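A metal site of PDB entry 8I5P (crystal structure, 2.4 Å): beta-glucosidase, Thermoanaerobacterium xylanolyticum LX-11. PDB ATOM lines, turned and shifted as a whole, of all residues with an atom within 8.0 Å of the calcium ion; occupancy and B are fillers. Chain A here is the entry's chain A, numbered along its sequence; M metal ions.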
ATOM      1  N   LYS A 557      -6.936 -13.382  25.364  1.00  0.00           N
ATOM      2  CA  LYS A 557      -8.086 -13.208  24.455  1.00  0.00           C
ATOM      3  C   LYS A 557      -8.607 -14.532  23.860  1.00  0.00           C
ATOM      4  O   LYS A 557      -9.826 -14.738  23.757  1.00  0.00           O
ATOM      5  CB  LYS A 557      -7.701 -12.264  23.308  1.00  0.00           C
ATOM      6  CG  LYS A 557      -8.823 -11.896  22.347  1.00  0.00           C
ATOM      7  CD  LYS A 557      -9.757 -10.837  22.926  1.00  0.00           C
ATOM      8  CE  LYS A 557     -10.711 -10.283  21.878  1.00  0.00           C
ATOM      9  NZ  LYS A 557     -11.810 -11.238  21.578  1.00  0.00           N
ATOM     10  N   MET A 559      -8.937 -17.236  25.287  1.00  0.00           N
ATOM     11  CA  MET A 559      -9.742 -17.939  26.304  1.00  0.00           C
ATOM     12  C   MET A 559     -11.181 -17.406  26.441  1.00  0.00           C
ATOM     13  O   MET A 559     -11.953 -17.880  27.280  1.00  0.00           O
ATOM     14  CB  MET A 559      -9.009 -17.935  27.648  1.00  0.00           C
ATOM     15  CG  MET A 559      -7.806 -18.859  27.644  1.00  0.00           C
ATOM     16  SD  MET A 559      -6.617 -18.498  28.936  1.00  0.00           S
ATOM     17  CE  MET A 559      -5.229 -19.493  28.391  1.00  0.00           C
ATOM     18  N   ASP A 560     -11.520 -16.419  25.616  1.00  0.00           N
ATOM     19  CA  ASP A 560     -12.898 -15.969  25.439  1.00  0.00           C
ATOM     20  C   ASP A 560     -13.725 -16.963  24.593  1.00  0.00           C
ATOM     21  O   ASP A 560     -13.656 -16.957  23.356  1.00  0.00           O
ATOM     22  CB  ASP A 560     -12.900 -14.581  24.806  1.00  0.00           C
ATOM     23  CG  ASP A 560     -14.283 -13.992  24.681  1.00  0.00           C
ATOM     24  OD1 ASP A 560     -15.229 -14.494  25.329  1.00  0.00           O
ATOM     25  OD2 ASP A 560     -14.420 -13.002  23.921  1.00  0.00           O
ATOM     26  N   LYS A 561     -14.487 -17.804  25.277  1.00  0.00           N
ATOM     27  CA  LYS A 561     -15.299 -18.864  24.653  1.00  0.00           C
ATOM     28  C   LYS A 561     -16.574 -18.309  24.021  1.00  0.00           C
ATOM     29  O   LYS A 561     -16.807 -18.490  22.836  1.00  0.00           O
ATOM     30  CB  LYS A 561     -15.695 -19.926  25.696  1.00  0.00           C
ATOM     31  CG  LYS A 561     -14.551 -20.608  26.442  1.00  0.00           C
ATOM     32  CD  LYS A 561     -13.669 -21.443  25.534  1.00  0.00           C
ATOM     33  CE  LYS A 561     -12.397 -20.703  25.119  1.00  0.00           C
ATOM     34  NZ  LYS A 561     -11.480 -21.568  24.325  1.00  0.00           N
ATOM     35  N   ASP A 562     -17.368 -17.608  24.827  1.00  0.00           N
ATOM     36  CA  ASP A 562     -18.699 -17.106  24.408  1.00  0.00           C
ATOM     37  C   ASP A 562     -18.686 -15.809  23.559  1.00  0.00           C
ATOM     38  O   ASP A 562     -19.747 -15.280  23.215  1.00  0.00           O
ATOM     39  CB  ASP A 562     -19.617 -16.953  25.627  1.00  0.00           C
ATOM     40  CG  ASP A 562     -19.054 -16.035  26.718  1.00  0.00           C
ATOM     41  OD1 ASP A 562     -18.294 -15.109  26.390  1.00  0.00           O
ATOM     42  OD2 ASP A 562     -19.365 -16.250  27.904  1.00  0.00           O
ATOM     43  N   ASN A 563     -17.499 -15.319  23.229  1.00  0.00           N
ATOM     44  CA  ASN A 563     -17.307 -14.108  22.411  1.00  0.00           C
ATOM     45  C   ASN A 563     -17.954 -12.816  22.981  1.00  0.00           C
ATOM     46  O   ASN A 563     -18.537 -12.025  22.241  1.00  0.00           O
ATOM     47  CB  ASN A 563     -17.738 -14.368  20.953  1.00  0.00           C
ATOM     48  CG  ASN A 563     -16.935 -13.535  19.943  1.00  0.00           C
ATOM     49  OD1 ASN A 563     -15.699 -13.591  19.919  1.00  0.00           O
ATOM     50  ND2 ASN A 563     -17.629 -12.763  19.110  1.00  0.00           N
ATOM     51  N   ASP A 564     -17.816 -12.609  24.289  1.00  0.00           N
ATOM     52  CA  ASP A 564     -18.190 -11.326  24.908  1.00  0.00           C
ATOM     53  C   ASP A 564     -17.000 -10.363  25.072  1.00  0.00           C
ATOM     54  O   ASP A 564     -17.150  -9.282  25.648  1.00  0.00           O
ATOM     55  CB  ASP A 564     -18.931 -11.531  26.236  1.00  0.00           C
ATOM     56  CG  ASP A 564     -18.054 -12.117  27.342  1.00  0.00           C
ATOM     57  OD1 ASP A 564     -16.908 -12.526  27.071  1.00  0.00           O
ATOM     58  OD2 ASP A 564     -18.526 -12.190  28.492  1.00  0.00           O
ATOM     59  N   GLY A 565     -15.838 -10.745  24.545  1.00  0.00           N
ATOM     60  CA  GLY A 565     -14.609  -9.933  24.644  1.00  0.00           C
ATOM     61  C   GLY A 565     -13.804 -10.114  25.932  1.00  0.00           C
ATOM     62  O   GLY A 565     -12.764  -9.485  26.089  1.00  0.00           O
ATOM     63  N   ILE A 566     -14.282 -10.977  26.836  1.00  0.00           N
ATOM     64  CA  ILE A 566     -13.668 -11.193  28.152  1.00  0.00           C
ATOM     65  C   ILE A 566     -13.242 -12.652  28.240  1.00  0.00           C
ATOM     66  O   ILE A 566     -13.940 -13.526  27.746  1.00  0.00           O
ATOM     67  CB  ILE A 566     -14.665 -10.874  29.295  1.00  0.00           C
ATOM     68  CG1 ILE A 566     -15.203  -9.436  29.163  1.00  0.00           C
ATOM     69  CG2 ILE A 566     -14.002 -11.030  30.656  1.00  0.00           C
ATOM     70  CD1 ILE A 566     -16.448  -9.145  29.982  1.00  0.00           C
ATOM     71  N   PRO A 567     -12.080 -12.943  28.862  1.00  0.00           N
ATOM     72  CA  PRO A 567     -11.729 -14.339  29.145  1.00  0.00           C
ATOM     73  C   PRO A 567     -12.758 -15.023  30.056  1.00  0.00           C
ATOM     74  O   PRO A 567     -13.259 -14.404  30.989  1.00  0.00           O
ATOM     75  CB  PRO A 567     -10.377 -14.223  29.851  1.00  0.00           C
ATOM     76  CG  PRO A 567      -9.814 -12.931  29.402  1.00  0.00           C
ATOM     77  CD  PRO A 567     -10.976 -12.015  29.194  1.00  0.00           C
ATOM     78  N   ASP A 568     -13.059 -16.290  29.750  1.00  0.00           N
ATOM     79  CA  ASP A 568     -13.993 -17.091  30.535  1.00  0.00           C
ATOM     80  C   ASP A 568     -13.246 -17.863  31.610  1.00  0.00           C
ATOM     81  O   ASP A 568     -12.303 -18.586  31.308  1.00  0.00           O
ATOM     82  CB  ASP A 568     -14.703 -18.134  29.656  1.00  0.00           C
ATOM     83  CG  ASP A 568     -15.717 -17.512  28.745  1.00  0.00           C
ATOM     84  OD1 ASP A 568     -15.308 -17.008  27.672  1.00  0.00           O
ATOM     85  OD2 ASP A 568     -16.923 -17.526  29.081  1.00  0.00           O
ATOM     86  N   ASN A 569     -13.677 -17.723  32.852  1.00  0.00           N
ATOM     87  CA  ASN A 569     -13.273 -18.629  33.907  1.00  0.00           C
ATOM     88  C   ASN A 569     -14.000 -19.944  33.661  1.00  0.00           C
ATOM     89  O   ASN A 569     -15.170 -19.938  33.270  1.00  0.00           O
ATOM     90  CB  ASN A 569     -13.579 -18.031  35.279  1.00  0.00           C
ATOM     91  CG  ASN A 569     -12.745 -16.797  35.580  1.00  0.00           C
ATOM     92  OD1 ASN A 569     -13.250 -15.683  35.609  1.00  0.00           O
ATOM     93  ND2 ASN A 569     -11.455 -16.999  35.780  1.00  0.00           N
ATOM     94  N   GLY A 584     -17.538 -18.330  33.987  1.00  0.00           N
ATOM     95  CA  GLY A 584     -18.072 -17.281  33.133  1.00  0.00           C
ATOM     96  C   GLY A 584     -17.221 -16.040  33.190  1.00  0.00           C
ATOM     97  O   GLY A 584     -15.995 -16.124  33.320  1.00  0.00           O
ATOM     98  N   THR A 585     -17.859 -14.879  33.079  1.00  0.00           N
ATOM     99  CA  THR A 585     -17.186 -13.613  33.351  1.00  0.00           C
ATOM    100  C   THR A 585     -17.223 -13.389  34.869  1.00  0.00           C
ATOM    101  O   THR A 585     -18.302 -13.380  35.469  1.00  0.00           O
ATOM    102  CB  THR A 585     -17.897 -12.446  32.643  1.00  0.00           C
ATOM    103  OG1 THR A 585     -17.775 -12.594  31.227  1.00  0.00           O
ATOM    104  CG2 THR A 585     -17.299 -11.095  33.048  1.00  0.00           C
ATOM    105  N   SER A 586     -16.036 -13.211  35.465  1.00  0.00           N
ATOM    106  CA  SER A 586     -15.900 -12.875  36.893  1.00  0.00           C
ATOM    107  C   SER A 586     -15.552 -11.399  37.100  1.00  0.00           C
ATOM    108  O   SER A 586     -14.909 -10.777  36.249  1.00  0.00           O
ATOM    109  CB  SER A 586     -14.851 -13.746  37.564  1.00  0.00           C
ATOM    110  OG  SER A 586     -13.571 -13.513  37.003  1.00  0.00           O
ATOM    111  N   TRP A 593      -8.676  -7.761  33.497  1.00  0.00           N
ATOM    112  CA  TRP A 593      -8.632  -7.740  32.023  1.00  0.00           C
ATOM    113  C   TRP A 593      -8.898  -6.339  31.460  1.00  0.00           C
ATOM    114  O   TRP A 593      -8.112  -5.823  30.656  1.00  0.00           O
ATOM    115  CB  TRP A 593      -9.622  -8.774  31.476  1.00  0.00           C
ATOM    116  CG  TRP A 593      -9.787  -8.822  29.975  1.00  0.00           C
ATOM    117  CD1 TRP A 593     -10.926  -8.547  29.270  1.00  0.00           C
ATOM    118  CD2 TRP A 593      -8.797  -9.184  29.013  1.00  0.00           C
ATOM    119  NE1 TRP A 593     -10.708  -8.720  27.937  1.00  0.00           N
ATOM    120  CE2 TRP A 593      -9.405  -9.106  27.735  1.00  0.00           C
ATOM    121  CE3 TRP A 593      -7.446  -9.558  29.099  1.00  0.00           C
ATOM    122  CZ2 TRP A 593      -8.724  -9.389  26.564  1.00  0.00           C
ATOM    123  CZ3 TRP A 593      -6.765  -9.842  27.927  1.00  0.00           C
ATOM    124  CH2 TRP A 593      -7.403  -9.743  26.671  1.00  0.00           C
ATOM    125  N   ASN A 626     -19.831  -5.170  27.971  1.00  0.00           N
ATOM    126  CA  ASN A 626     -20.291  -6.513  28.370  1.00  0.00           C
ATOM    127  C   ASN A 626     -20.080  -6.816  29.863  1.00  0.00           C
ATOM    128  O   ASN A 626     -20.910  -7.484  30.492  1.00  0.00           O
ATOM    129  CB  ASN A 626     -19.632  -7.591  27.491  1.00  0.00           C
ATOM    130  CG  ASN A 626     -20.252  -7.680  26.099  1.00  0.00           C
ATOM    131  OD1 ASN A 626     -21.475  -7.767  25.969  1.00  0.00           O
ATOM    132  ND2 ASN A 626     -19.428  -7.695  25.061  1.00  0.00           N
ATOM    133  N   GLU A 630     -23.198  -7.718  32.185  1.00  0.00           N
ATOM    134  CA  GLU A 630     -23.203  -9.060  32.800  1.00  0.00           C
ATOM    135  C   GLU A 630     -23.177  -9.072  34.337  1.00  0.00           C
ATOM    136  O   GLU A 630     -23.748  -9.990  34.934  1.00  0.00           O
ATOM    137  CB  GLU A 630     -22.041  -9.887  32.260  1.00  0.00           C
ATOM    138  CG  GLU A 630     -22.207 -10.314  30.794  1.00  0.00           C
ATOM    139  CD  GLU A 630     -20.916 -10.801  30.158  1.00  0.00           C
ATOM    140  OE1 GLU A 630     -20.010 -11.255  30.887  1.00  0.00           O
ATOM    141  OE2 GLU A 630     -20.820 -10.738  28.920  1.00  0.00           O
ATOM    142  N   THR A 641     -20.812 -14.784  36.478  1.00  0.00           N
ATOM    143  CA  THR A 641     -22.049 -15.089  35.724  1.00  0.00           C
ATOM    144  C   THR A 641     -22.571 -16.547  35.818  1.00  0.00           C
ATOM    145  O   THR A 641     -23.770 -16.763  35.661  1.00  0.00           O
ATOM    146  CB  THR A 641     -21.887 -14.741  34.231  1.00  0.00           C
ATOM    147  OG1 THR A 641     -20.822 -15.522  33.663  1.00  0.00           O
ATOM    148  CG2 THR A 641     -21.588 -13.257  34.024  1.00  0.00           C
ATOM    149  N   GLU A 642     -21.698 -17.520  36.076  1.00  0.00           N
ATOM    150  CA  GLU A 642     -22.084 -18.954  36.005  1.00  0.00           C
ATOM    151  C   GLU A 642     -21.868 -19.819  37.259  1.00  0.00           C
ATOM    152  O   GLU A 642     -22.120 -21.031  37.209  1.00  0.00           O
ATOM    153  CB  GLU A 642     -21.385 -19.627  34.815  1.00  0.00           C
ATOM    154  CG  GLU A 642     -21.774 -19.099  33.444  1.00  0.00           C
ATOM    155  CD  GLU A 642     -21.217 -19.947  32.305  1.00  0.00           C
ATOM    156  OE1 GLU A 642     -21.279 -21.193  32.392  1.00  0.00           O
ATOM    157  OE2 GLU A 642     -20.709 -19.370  31.311  1.00  0.00           O
HETATM  158 CA    CA M   1     -16.050 -14.496  27.702  1.00  0.00          CA
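OD2 of Asp 564 sits at hydrogen-bond distance from OG1 of Thr 585 (2.9 Å).
The side-chain carboxylate (OD2) of Asp 564 sits close to the side-chain carboxylate (OE2) of Glu 630, at 2.7 Å.
The backbone carbonyl oxygen (O) of Asp 564 is in hydrogen-bond range of the side-chain amide nitrogen (ND2) of Asn 626.
The side-chain carboxylate (OD1) of Asp 560 sits close to the backbone NH (N) of Asn 563 (3.2 Å).
OD2 of Asp 560 sits at hydrogen-bond distance from N of Gly 565 (2.7 Å).
The side-chain carboxylate (OD2) of Asp 560 lies within salt-bridge range of the side-chain amino group (NZ) of Lys 557 (3.9 Å).
The side-chain carboxylate (OD1) of Asp 568 lies close to the backbone NH (N) of Lys 561 (2.7 Å).
O of Met 559 is in hydrogen-bond range of N of Asp 568 (3.1 Å).
The calcium ion is bound by OD1 of Asp 564, O of Ile 566, OD1 of Asp 560, OD1 of Asp 568 and OD1 of Asp 562.
The calcium ion has five donor atoms within binding distance.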
